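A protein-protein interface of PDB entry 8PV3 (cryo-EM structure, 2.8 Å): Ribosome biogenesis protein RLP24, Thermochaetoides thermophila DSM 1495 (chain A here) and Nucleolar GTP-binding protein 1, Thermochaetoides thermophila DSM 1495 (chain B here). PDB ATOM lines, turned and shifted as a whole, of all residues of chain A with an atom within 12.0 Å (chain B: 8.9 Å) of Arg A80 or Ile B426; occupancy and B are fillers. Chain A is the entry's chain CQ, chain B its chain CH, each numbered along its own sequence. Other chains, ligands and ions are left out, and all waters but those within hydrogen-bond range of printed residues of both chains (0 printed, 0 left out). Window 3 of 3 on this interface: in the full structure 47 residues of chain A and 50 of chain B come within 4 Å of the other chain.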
ATOM      1  N   ARG A  75      24.381  -7.381 -28.503  1.00  0.00           N
ATOM      2  CA  ARG A  75      23.821  -6.432 -29.456  1.00  0.00           C
ATOM      3  C   ARG A  75      24.052  -5.021 -28.932  1.00  0.00           C
ATOM      4  O   ARG A  75      23.369  -4.573 -28.006  1.00  0.00           O
ATOM      5  CB  ARG A  75      22.337  -6.708 -29.671  1.00  0.00           C
ATOM      6  CG  ARG A  75      22.012  -8.177 -29.860  1.00  0.00           C
ATOM      7  CD  ARG A  75      22.374  -8.650 -31.252  1.00  0.00           C
ATOM      8  NE  ARG A  75      22.209 -10.091 -31.399  1.00  0.00           N
ATOM      9  CZ  ARG A  75      22.258 -10.734 -32.556  1.00  0.00           C
ATOM     10  NH1 ARG A  75      22.449 -10.093 -33.697  1.00  0.00           N
ATOM     11  NH2 ARG A  75      22.106 -12.055 -32.571  1.00  0.00           N
ATOM     12  N   ASN A  76      25.015  -4.321 -29.525  1.00  0.00           N
ATOM     13  CA  ASN A  76      25.339  -2.960 -29.128  1.00  0.00           C
ATOM     14  C   ASN A  76      24.526  -1.913 -29.873  1.00  0.00           C
ATOM     15  O   ASN A  76      24.586  -0.734 -29.514  1.00  0.00           O
ATOM     16  CB  ASN A  76      26.832  -2.694 -29.335  1.00  0.00           C
ATOM     17  CG  ASN A  76      27.690  -3.328 -28.262  1.00  0.00           C
ATOM     18  OD1 ASN A  76      27.213  -3.639 -27.174  1.00  0.00           O
ATOM     19  ND2 ASN A  76      28.964  -3.521 -28.564  1.00  0.00           N
ATOM     20  N   VAL A  77      23.774  -2.311 -30.894  1.00  0.00           N
ATOM     21  CA  VAL A  77      22.870  -1.405 -31.594  1.00  0.00           C
ATOM     22  C   VAL A  77      21.444  -1.796 -31.233  1.00  0.00           C
ATOM     23  O   VAL A  77      20.980  -2.873 -31.636  1.00  0.00           O
ATOM     24  CB  VAL A  77      23.101  -1.443 -33.111  1.00  0.00           C
ATOM     25  CG1 VAL A  77      22.161  -0.479 -33.809  1.00  0.00           C
ATOM     26  CG2 VAL A  77      24.543  -1.104 -33.430  1.00  0.00           C
ATOM     27  N   PRO A  78      20.726  -0.976 -30.466  1.00  0.00           N
ATOM     28  CA  PRO A  78      19.374  -1.353 -30.042  1.00  0.00           C
ATOM     29  C   PRO A  78      18.381  -1.334 -31.194  1.00  0.00           C
ATOM     30  O   PRO A  78      18.537  -0.602 -32.173  1.00  0.00           O
ATOM     31  CB  PRO A  78      19.028  -0.293 -28.994  1.00  0.00           C
ATOM     32  CG  PRO A  78      19.850   0.880 -29.382  1.00  0.00           C
ATOM     33  CD  PRO A  78      21.139   0.313 -29.891  1.00  0.00           C
ATOM     34  N   VAL A  79      17.350  -2.161 -31.060  1.00  0.00           N
ATOM     35  CA  VAL A  79      16.261  -2.251 -32.023  1.00  0.00           C
ATOM     36  C   VAL A  79      14.999  -1.718 -31.360  1.00  0.00           C
ATOM     37  O   VAL A  79      14.739  -2.007 -30.186  1.00  0.00           O
ATOM     38  CB  VAL A  79      16.077  -3.703 -32.508  1.00  0.00           C
ATOM     39  CG1 VAL A  79      14.895  -3.828 -33.454  1.00  0.00           C
ATOM     40  CG2 VAL A  79      17.347  -4.201 -33.171  1.00  0.00           C
ATOM     41  N   ARG A  80      14.242  -0.902 -32.099  1.00  0.00           N
ATOM     42  CA  ARG A  80      12.957  -0.401 -31.625  1.00  0.00           C
ATOM     43  C   ARG A  80      12.011  -1.560 -31.337  1.00  0.00           C
ATOM     44  O   ARG A  80      11.977  -2.549 -32.072  1.00  0.00           O
ATOM     45  CB  ARG A  80      12.352   0.540 -32.668  1.00  0.00           C
ATOM     46  CG  ARG A  80      11.074   1.233 -32.240  1.00  0.00           C
ATOM     47  CD  ARG A  80      10.738   2.391 -33.161  1.00  0.00           C
ATOM     48  NE  ARG A  80      11.818   3.367 -33.222  1.00  0.00           N
ATOM     49  CZ  ARG A  80      11.983   4.360 -32.358  1.00  0.00           C
ATOM     50  NH1 ARG A  80      11.163   4.530 -31.337  1.00  0.00           N
ATOM     51  NH2 ARG A  80      13.002   5.198 -32.522  1.00  0.00           N
ATOM     52  N   TYR A  81      11.248  -1.439 -30.251  1.00  0.00           N
ATOM     53  CA  TYR A  81      10.506  -2.583 -29.739  1.00  0.00           C
ATOM     54  C   TYR A  81       9.327  -2.922 -30.643  1.00  0.00           C
ATOM     55  O   TYR A  81       8.540  -2.046 -31.015  1.00  0.00           O
ATOM     56  CB  TYR A  81      10.017  -2.318 -28.318  1.00  0.00           C
ATOM     57  CG  TYR A  81       8.972  -3.310 -27.877  1.00  0.00           C
ATOM     58  CD1 TYR A  81       9.314  -4.635 -27.655  1.00  0.00           C
ATOM     59  CD2 TYR A  81       7.651  -2.933 -27.691  1.00  0.00           C
ATOM     60  CE1 TYR A  81       8.378  -5.557 -27.259  1.00  0.00           C
ATOM     61  CE2 TYR A  81       6.702  -3.854 -27.294  1.00  0.00           C
ATOM     62  CZ  TYR A  81       7.075  -5.164 -27.083  1.00  0.00           C
ATOM     63  OH  TYR A  81       6.147  -6.092 -26.685  1.00  0.00           O
ATOM     64  N   ASN A  82       9.201  -4.203 -30.984  1.00  0.00           N
ATOM     65  CA  ASN A  82       8.164  -4.679 -31.889  1.00  0.00           C
ATOM     66  C   ASN A  82       7.661  -6.017 -31.367  1.00  0.00           C
ATOM     67  O   ASN A  82       8.439  -6.972 -31.248  1.00  0.00           O
ATOM     68  CB  ASN A  82       8.715  -4.802 -33.314  1.00  0.00           C
ATOM     69  CG  ASN A  82       7.629  -4.900 -34.361  1.00  0.00           C
ATOM     70  OD1 ASN A  82       6.643  -5.609 -34.196  1.00  0.00           O
ATOM     71  ND2 ASN A  82       7.804  -4.166 -35.453  1.00  0.00           N
ATOM     72  N   ARG A  83       6.354  -6.081 -31.080  1.00  0.00           N
ATOM     73  CA  ARG A  83       5.778  -7.242 -30.406  1.00  0.00           C
ATOM     74  C   ARG A  83       5.959  -8.516 -31.220  1.00  0.00           C
ATOM     75  O   ARG A  83       6.354  -9.556 -30.677  1.00  0.00           O
ATOM     76  CB  ARG A  83       4.297  -7.000 -30.125  1.00  0.00           C
ATOM     77  CG  ARG A  83       3.604  -8.165 -29.441  1.00  0.00           C
ATOM     78  CD  ARG A  83       2.121  -7.900 -29.256  1.00  0.00           C
ATOM     79  NE  ARG A  83       1.858  -6.819 -28.318  1.00  0.00           N
ATOM     80  CZ  ARG A  83       0.651  -6.334 -28.058  1.00  0.00           C
ATOM     81  NH1 ARG A  83      -0.425  -6.802 -28.668  1.00  0.00           N
ATOM     82  NH2 ARG A  83       0.522  -5.352 -27.173  1.00  0.00           N
ATOM     83  N   GLU A  84       5.707  -8.445 -32.531  1.00  0.00           N
ATOM     84  CA  GLU A  84       5.898  -9.610 -33.388  1.00  0.00           C
ATOM     85  C   GLU A  84       7.362 -10.025 -33.448  1.00  0.00           C
ATOM     86  O   GLU A  84       7.668 -11.219 -33.538  1.00  0.00           O
ATOM     87  CB  GLU A  84       5.368  -9.331 -34.794  1.00  0.00           C
ATOM     88  CG  GLU A  84       3.853  -9.262 -34.899  1.00  0.00           C
ATOM     89  CD  GLU A  84       3.309  -7.888 -34.587  1.00  0.00           C
ATOM     90  OE1 GLU A  84       4.120  -6.969 -34.369  1.00  0.00           O
ATOM     91  OE2 GLU A  84       2.071  -7.727 -34.561  1.00  0.00           O
ATOM     92  N   LEU A  85       8.281  -9.055 -33.382  1.00  0.00           N
ATOM     93  CA  LEU A  85       9.703  -9.377 -33.452  1.00  0.00           C
ATOM     94  C   LEU A  85      10.158 -10.147 -32.218  1.00  0.00           C
ATOM     95  O   LEU A  85      10.835 -11.172 -32.339  1.00  0.00           O
ATOM     96  CB  LEU A  85      10.526  -8.102 -33.629  1.00  0.00           C
ATOM     97  CG  LEU A  85      12.046  -8.259 -33.532  1.00  0.00           C
ATOM     98  CD1 LEU A  85      12.570  -9.142 -34.648  1.00  0.00           C
ATOM     99  CD2 LEU A  85      12.731  -6.910 -33.563  1.00  0.00           C
ATOM    100  N   TRP A  86       9.770  -9.687 -31.024  1.00  0.00           N
ATOM    101  CA  TRP A  86      10.024 -10.468 -29.808  1.00  0.00           C
ATOM    102  C   TRP A  86       9.331 -11.833 -29.799  1.00  0.00           C
ATOM    103  O   TRP A  86       9.933 -12.820 -29.352  1.00  0.00           O
ATOM    104  CB  TRP A  86       9.689  -9.634 -28.570  1.00  0.00           C
ATOM    105  CG  TRP A  86      10.838  -8.764 -28.081  1.00  0.00           C
ATOM    106  CD1 TRP A  86      11.662  -9.060 -27.034  1.00  0.00           C
ATOM    107  CD2 TRP A  86      11.428  -7.625 -28.724  1.00  0.00           C
ATOM    108  NE1 TRP A  86      12.636  -8.108 -26.903  1.00  0.00           N
ATOM    109  CE2 TRP A  86      12.527  -7.223 -27.939  1.00  0.00           C
ATOM    110  CE3 TRP A  86      11.109  -6.876 -29.854  1.00  0.00           C
ATOM    111  CZ2 TRP A  86      13.303  -6.113 -28.253  1.00  0.00           C
ATOM    112  CZ3 TRP A  86      11.880  -5.781 -30.163  1.00  0.00           C
ATOM    113  CH2 TRP A  86      12.959  -5.403 -29.365  1.00  0.00           C
ATOM    114  N   GLN A  87       8.089 -11.937 -30.290  1.00  0.00           N
ATOM    115  CA  GLN A  87       7.432 -13.249 -30.285  1.00  0.00           C
ATOM    116  C   GLN A  87       8.127 -14.241 -31.221  1.00  0.00           C
ATOM    117  O   GLN A  87       8.403 -15.393 -30.835  1.00  0.00           O
ATOM    118  CB  GLN A  87       5.955 -13.115 -30.652  1.00  0.00           C
ATOM    119  CG  GLN A  87       5.132 -12.298 -29.672  1.00  0.00           C
ATOM    120  CD  GLN A  87       5.235 -12.803 -28.248  1.00  0.00           C
ATOM    121  OE1 GLN A  87       5.900 -12.196 -27.411  1.00  0.00           O
ATOM    122  NE2 GLN A  87       4.569 -13.916 -27.963  1.00  0.00           N
ATOM    123  N   LYS A  88       8.440 -13.812 -32.448  1.00  0.00           N
ATOM    124  CA  LYS A  88       9.130 -14.710 -33.366  1.00  0.00           C
ATOM    125  C   LYS A  88      10.563 -14.965 -32.923  1.00  0.00           C
ATOM    126  O   LYS A  88      11.118 -16.024 -33.227  1.00  0.00           O
ATOM    127  CB  LYS A  88       9.081 -14.166 -34.793  1.00  0.00           C
ATOM    128  CG  LYS A  88       9.971 -12.977 -35.076  1.00  0.00           C
ATOM    129  CD  LYS A  88       9.861 -12.569 -36.533  1.00  0.00           C
ATOM    130  CE  LYS A  88       8.566 -11.821 -36.800  1.00  0.00           C
ATOM    131  NZ  LYS A  88       8.554 -11.183 -38.146  1.00  0.00           N
ATOM    132  N   THR A  89      11.160 -14.042 -32.160  1.00  0.00           N
ATOM    133  CA  THR A  89      12.470 -14.301 -31.576  1.00  0.00           C
ATOM    134  C   THR A  89      12.393 -15.395 -30.521  1.00  0.00           C
ATOM    135  O   THR A  89      13.293 -16.234 -30.427  1.00  0.00           O
ATOM    136  CB  THR A  89      13.040 -13.013 -30.987  1.00  0.00           C
ATOM    137  OG1 THR A  89      13.025 -11.990 -31.990  1.00  0.00           O
ATOM    138  CG2 THR A  89      14.471 -13.220 -30.522  1.00  0.00           C
ATOM    139  N   LEU B 421       7.438   6.551 -17.710  1.00  0.00           N
ATOM    140  CA  LEU B 421       8.555   6.644 -18.639  1.00  0.00           C
ATOM    141  C   LEU B 421       8.207   6.164 -20.040  1.00  0.00           C
ATOM    142  O   LEU B 421       8.876   6.566 -20.998  1.00  0.00           O
ATOM    143  CB  LEU B 421       9.746   5.844 -18.107  1.00  0.00           C
ATOM    144  CG  LEU B 421      10.323   6.308 -16.771  1.00  0.00           C
ATOM    145  CD1 LEU B 421      11.454   5.396 -16.330  1.00  0.00           C
ATOM    146  CD2 LEU B 421      10.797   7.746 -16.867  1.00  0.00           C
ATOM    147  N   ARG B 422       7.181   5.332 -20.186  1.00  0.00           N
ATOM    148  CA  ARG B 422       6.796   4.782 -21.476  1.00  0.00           C
ATOM    149  C   ARG B 422       5.801   5.660 -22.220  1.00  0.00           C
ATOM    150  O   ARG B 422       5.341   5.270 -23.295  1.00  0.00           O
ATOM    151  CB  ARG B 422       6.208   3.379 -21.295  1.00  0.00           C
ATOM    152  CG  ARG B 422       7.247   2.307 -21.037  1.00  0.00           C
ATOM    153  CD  ARG B 422       6.663   1.161 -20.244  1.00  0.00           C
ATOM    154  NE  ARG B 422       7.616   0.073 -20.069  1.00  0.00           N
ATOM    155  CZ  ARG B 422       7.547  -1.093 -20.693  1.00  0.00           C
ATOM    156  NH1 ARG B 422       6.579  -1.359 -21.553  1.00  0.00           N
ATOM    157  NH2 ARG B 422       8.470  -2.017 -20.445  1.00  0.00           N
ATOM    158  N   LYS B 423       5.453   6.824 -21.669  1.00  0.00           N
ATOM    159  CA  LYS B 423       4.450   7.679 -22.297  1.00  0.00           C
ATOM    160  C   LYS B 423       4.966   8.295 -23.590  1.00  0.00           C
ATOM    161  O   LYS B 423       4.213   8.440 -24.559  1.00  0.00           O
ATOM    162  CB  LYS B 423       4.014   8.772 -21.323  1.00  0.00           C
ATOM    163  CG  LYS B 423       2.732   9.475 -21.715  1.00  0.00           C
ATOM    164  CD  LYS B 423       1.983   9.970 -20.495  1.00  0.00           C
ATOM    165  CE  LYS B 423       2.557  11.287 -20.000  1.00  0.00           C
ATOM    166  NZ  LYS B 423       2.638  12.299 -21.088  1.00  0.00           N
ATOM    167  N   ASP B 424       6.246   8.663 -23.629  1.00  0.00           N
ATOM    168  CA  ASP B 424       6.837   9.304 -24.794  1.00  0.00           C
ATOM    169  C   ASP B 424       7.569   8.321 -25.699  1.00  0.00           C
ATOM    170  O   ASP B 424       8.417   8.737 -26.493  1.00  0.00           O
ATOM    171  CB  ASP B 424       7.779  10.426 -24.360  1.00  0.00           C
ATOM    172  CG  ASP B 424       7.042  11.598 -23.749  1.00  0.00           C
ATOM    173  OD1 ASP B 424       5.876  11.829 -24.130  1.00  0.00           O
ATOM    174  OD2 ASP B 424       7.627  12.291 -22.890  1.00  0.00           O
ATOM    175  N   TRP B 425       7.265   7.032 -25.591  1.00  0.00           N
ATOM    176  CA  TRP B 425       7.832   6.054 -26.507  1.00  0.00           C
ATOM    177  C   TRP B 425       7.245   6.236 -27.899  1.00  0.00           C
ATOM    178  O   TRP B 425       6.053   6.508 -28.058  1.00  0.00           O
ATOM    179  CB  TRP B 425       7.566   4.637 -26.007  1.00  0.00           C
ATOM    180  CG  TRP B 425       8.601   4.124 -25.062  1.00  0.00           C
ATOM    181  CD1 TRP B 425       9.572   4.850 -24.436  1.00  0.00           C
ATOM    182  CD2 TRP B 425       8.777   2.770 -24.637  1.00  0.00           C
ATOM    183  NE1 TRP B 425      10.339   4.032 -23.646  1.00  0.00           N
ATOM    184  CE2 TRP B 425       9.872   2.749 -23.751  1.00  0.00           C
ATOM    185  CE3 TRP B 425       8.115   1.571 -24.919  1.00  0.00           C
ATOM    186  CZ2 TRP B 425      10.319   1.579 -23.146  1.00  0.00           C
ATOM    187  CZ3 TRP B 425       8.559   0.411 -24.317  1.00  0.00           C
ATOM    188  CH2 TRP B 425       9.651   0.423 -23.442  1.00  0.00           C
ATOM    189  N   ILE B 426       8.090   6.088 -28.911  1.00  0.00           N
ATOM    190  CA  ILE B 426       7.684   6.192 -30.307  1.00  0.00           C
ATOM    191  C   ILE B 426       7.743   4.793 -30.896  1.00  0.00           C
ATOM    192  O   ILE B 426       8.827   4.280 -31.193  1.00  0.00           O
ATOM    193  CB  ILE B 426       8.575   7.161 -31.092  1.00  0.00           C
ATOM    194  CG1 ILE B 426       8.601   8.532 -30.417  1.00  0.00           C
ATOM    195  CG2 ILE B 426       8.084   7.286 -32.522  1.00  0.00           C
ATOM    196  CD1 ILE B 426       9.690   9.437 -30.935  1.00  0.00           C
ATOM    197  N   LEU B 427       6.583   4.172 -31.070  1.00  0.00           N
ATOM    198  CA  LEU B 427       6.505   2.809 -31.563  1.00  0.00           C
ATOM    199  C   LEU B 427       5.658   2.760 -32.825  1.00  0.00           C
ATOM    200  O   LEU B 427       4.899   3.684 -33.123  1.00  0.00           O
ATOM    201  CB  LEU B 427       5.926   1.865 -30.503  1.00  0.00           C
ATOM    202  CG  LEU B 427       6.693   1.781 -29.183  1.00  0.00           C
ATOM    203  CD1 LEU B 427       6.043   0.771 -28.269  1.00  0.00           C
ATOM    204  CD2 LEU B 427       8.154   1.429 -29.409  1.00  0.00           C
ATOM    205  N   GLU B 428       5.821   1.666 -33.573  1.00  0.00           N
ATOM    206  CA  GLU B 428       5.044   1.468 -34.794  1.00  0.00           C
ATOM    207  C   GLU B 428       3.556   1.366 -34.489  1.00  0.00           C
ATOM    208  O   GLU B 428       2.725   1.935 -35.206  1.00  0.00           O
ATOM    209  CB  GLU B 428       5.531   0.216 -35.522  1.00  0.00           C
ATOM    210  CG  GLU B 428       4.842  -0.041 -36.848  1.00  0.00           C
ATOM    211  CD  GLU B 428       5.389  -1.260 -37.558  1.00  0.00           C
ATOM    212  OE1 GLU B 428       6.297  -1.915 -37.003  1.00  0.00           O
ATOM    213  OE2 GLU B 428       4.913  -1.565 -38.672  1.00  0.00           O
ATOM    214  N   ASN B 429       3.203   0.648 -33.427  1.00  0.00           N
ATOM    215  CA  ASN B 429       1.835   0.586 -32.933  1.00  0.00           C
ATOM    216  C   ASN B 429       1.819   1.132 -31.513  1.00  0.00           C
ATOM    217  O   ASN B 429       2.501   0.573 -30.636  1.00  0.00           O
ATOM    218  CB  ASN B 429       1.305  -0.848 -32.971  1.00  0.00           C
ATOM    219  CG  ASN B 429      -0.175  -0.936 -32.656  1.00  0.00           C
ATOM    220  OD1 ASN B 429      -0.872   0.074 -32.590  1.00  0.00           O
ATOM    221  ND2 ASN B 429      -0.663  -2.153 -32.458  1.00  0.00           N
ATOM    222  N   PRO B 430       1.084   2.214 -31.234  1.00  0.00           N
ATOM    223  CA  PRO B 430       1.068   2.767 -29.868  1.00  0.00           C
ATOM    224  C   PRO B 430       0.424   1.855 -28.836  1.00  0.00           C
ATOM    225  O   PRO B 430       0.592   2.094 -27.634  1.00  0.00           O
ATOM    226  CB  PRO B 430       0.278   4.072 -30.027  1.00  0.00           C
ATOM    227  CG  PRO B 430       0.386   4.409 -31.477  1.00  0.00           C
ATOM    228  CD  PRO B 430       0.392   3.094 -32.188  1.00  0.00           C
ATOM    229  N   TRP B 432       1.436  -1.021 -28.199  1.00  0.00           N
ATOM    230  CA  TRP B 432       2.541  -1.776 -27.630  1.00  0.00           C
ATOM    231  C   TRP B 432       3.321  -0.996 -26.583  1.00  0.00           C
ATOM    232  O   TRP B 432       4.336  -1.499 -26.091  1.00  0.00           O
ATOM    233  CB  TRP B 432       3.507  -2.217 -28.733  1.00  0.00           C
ATOM    234  CG  TRP B 432       2.894  -2.999 -29.845  1.00  0.00           C
ATOM    235  CD1 TRP B 432       1.731  -3.709 -29.812  1.00  0.00           C
ATOM    236  CD2 TRP B 432       3.421  -3.151 -31.166  1.00  0.00           C
ATOM    237  NE1 TRP B 432       1.501  -4.295 -31.031  1.00  0.00           N
ATOM    238  CE2 TRP B 432       2.525  -3.968 -31.880  1.00  0.00           C
ATOM    239  CE3 TRP B 432       4.565  -2.676 -31.812  1.00  0.00           C
ATOM    240  CZ2 TRP B 432       2.735  -4.317 -33.209  1.00  0.00           C
ATOM    241  CZ3 TRP B 432       4.771  -3.025 -33.129  1.00  0.00           C
ATOM    242  CH2 TRP B 432       3.863  -3.836 -33.816  1.00  0.00           C
ATOM    243  N   LYS B 433       2.887   0.219 -26.236  1.00  0.00           N
ATOM    244  CA  LYS B 433       3.696   1.083 -25.384  1.00  0.00           C
ATOM    245  C   LYS B 433       3.763   0.605 -23.941  1.00  0.00           C
ATOM    246  O   LYS B 433       4.688   0.990 -23.219  1.00  0.00           O
ATOM    247  CB  LYS B 433       3.166   2.517 -25.429  1.00  0.00           C
ATOM    248  CG  LYS B 433       4.005   3.448 -26.286  1.00  0.00           C
ATOM    249  CD  LYS B 433       3.263   4.726 -26.629  1.00  0.00           C
ATOM    250  CE  LYS B 433       2.798   5.454 -25.384  1.00  0.00           C
ATOM    251  NZ  LYS B 433       2.259   6.801 -25.710  1.00  0.00           N
ATOM    252  N   ILE B 437       8.063  -6.442 -21.941  1.00  0.00           N
ATOM    253  CA  ILE B 437       9.031  -6.950 -22.909  1.00  0.00           C
ATOM    254  C   ILE B 437       9.738  -8.154 -22.299  1.00  0.00           C
ATOM    255  O   ILE B 437      10.303  -8.041 -21.203  1.00  0.00           O
ATOM    256  CB  ILE B 437      10.035  -5.859 -23.313  1.00  0.00           C
ATOM    257  CG1 ILE B 437       9.295  -4.629 -23.836  1.00  0.00           C
ATOM    258  CG2 ILE B 437      10.983  -6.383 -24.373  1.00  0.00           C
ATOM    259  CD1 ILE B 437      10.195  -3.441 -24.073  1.00  0.00           C
ATOM    260  N   TYR B 447      17.286 -10.478 -25.549  1.00  0.00           N
ATOM    261  CA  TYR B 447      17.924  -9.342 -26.203  1.00  0.00           C
ATOM    262  C   TYR B 447      19.168  -9.758 -26.973  1.00  0.00           C
ATOM    263  O   TYR B 447      19.484  -9.156 -28.004  1.00  0.00           O
ATOM    264  CB  TYR B 447      18.280  -8.276 -25.172  1.00  0.00           C
ATOM    265  CG  TYR B 447      17.118  -7.399 -24.771  1.00  0.00           C
ATOM    266  CD1 TYR B 447      16.132  -7.868 -23.914  1.00  0.00           C
ATOM    267  CD2 TYR B 447      17.008  -6.102 -25.250  1.00  0.00           C
ATOM    268  CE1 TYR B 447      15.071  -7.070 -23.545  1.00  0.00           C
ATOM    269  CE2 TYR B 447      15.951  -5.296 -24.886  1.00  0.00           C
ATOM    270  CZ  TYR B 447      14.987  -5.785 -24.034  1.00  0.00           C
ATOM    271  OH  TYR B 447      13.932  -4.983 -23.669  1.00  0.00           O
ATOM    272  N   ILE B 450      17.699 -10.964 -30.231  1.00  0.00           N
ATOM    273  CA  ILE B 450      16.951 -10.028 -31.067  1.00  0.00           C
ATOM    274  C   ILE B 450      17.789  -9.657 -32.279  1.00  0.00           C
ATOM    275  O   ILE B 450      18.919  -9.173 -32.150  1.00  0.00           O
ATOM    276  CB  ILE B 450      16.539  -8.787 -30.268  1.00  0.00           C
ATOM    277  CG1 ILE B 450      15.430  -9.137 -29.283  1.00  0.00           C
ATOM    278  CG2 ILE B 450      16.080  -7.677 -31.199  1.00  0.00           C
ATOM    279  CD1 ILE B 450      14.152  -9.564 -29.950  1.00  0.00           C
ATOM    280  N   PRO B 452      16.906  -8.037 -36.319  1.00  0.00           N
ATOM    281  CA  PRO B 452      15.852  -7.604 -37.259  1.00  0.00           C
ATOM    282  C   PRO B 452      15.646  -8.535 -38.444  1.00  0.00           C
ATOM    283  O   PRO B 452      14.499  -8.759 -38.853  1.00  0.00           O
ATOM    284  CB  PRO B 452      16.336  -6.217 -37.710  1.00  0.00           C
ATOM    285  CG  PRO B 452      17.771  -6.130 -37.285  1.00  0.00           C
ATOM    286  CD  PRO B 452      17.886  -6.971 -36.065  1.00  0.00           C
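The guanidinium group (NH1) of Arg A80 lies close to the backbone carbonyl oxygen (O) of Ile B426, at 2.4 Å.
NE of Arg A75 is in hydrogen-bond range of O of Ile B450.
The side-chain amide nitrogen of Asn A82 is in hydrogen-bond range of the side-chain carboxylate of Glu B428, at 3.1 Å.
The indole nitrogen (NE1) of Trp B432 lies close to the side-chain amide nitrogen (ND2) of Asn B429, at 3.4 Å.
OD1 of Asn A82 lies close to OE1 of Glu A84 (2.9 Å).
CG of Arg A75 touches O of Tyr B447 (3.3 Å).
Tyr A81 touches Leu B427.
Tyr A81 touches Trp B432 (CE2 to O, 3.5 Å).
Ile B437 touches Tyr A81.
Asn A82 touches Trp B432 (OD1 to CH2, 3.3 Å).
Trp B432 touches Arg A83.
OE1 of Glu A84 touches CH2 of Trp B432, at 3.2 Å.
CG2 of Ile B437 touches NE1 of Trp A86 (3.5 Å).
CD1 of Ile B450 touches CE2 of Trp A86, at 3.5 Å.
OG1 of Thr A89 touches CD1 of Ile B450, at 3.4 Å.
Arg A80 touches just one residue of chain B: Ile B426.
Ile B426 touches just one residue of chain A: Arg A80.
No residue of chain B comes within 4 Å of Val A79.
Of the printed residues of chain A, Leu B427 touches Tyr A81 (3.8 Å).
Of the printed residues of chain B, Arg A83 touches Trp B432 (3.3 Å).
Printed residues of chain A within 4 Å of Glu B428: Asn A82.
Printed residues of chain B within 4 Å of Asn A82: Glu B428 and Trp B432.
Of the printed residues of chain A, Trp B432 touches Tyr A81, Asn A82, Arg A83 and Glu A84.
Of the printed residues of chain A, Ile B437 touches Tyr A81 (3.7 Å) and Trp A86 (3.5 Å).
Arg B422 touches none of the printed residues of chain A.
Lys A88 touches none of the printed residues of chain B.
The nearest residue of chain B that does not touch Arg A80 is Leu B427 (4.1 Å).
Printed residues of chain A that touch a printed residue of chain B: Arg A75, Arg A80, Tyr A81, Asn A82, Arg A83, Glu A84, Trp A86 and Thr A89.
Hydrophobic or aromatic side chains of chain A that line the printed part of chain B: Tyr A81 and Trp A86.
Along chain A the printed residues that touch a printed residue of chain B span positions 75 to 89.
Printed residues of chain B that touch a printed residue of chain A: Ile B426, Leu B427, Glu B428, Trp B432, Ile B437, Tyr B447 and Ile B450.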
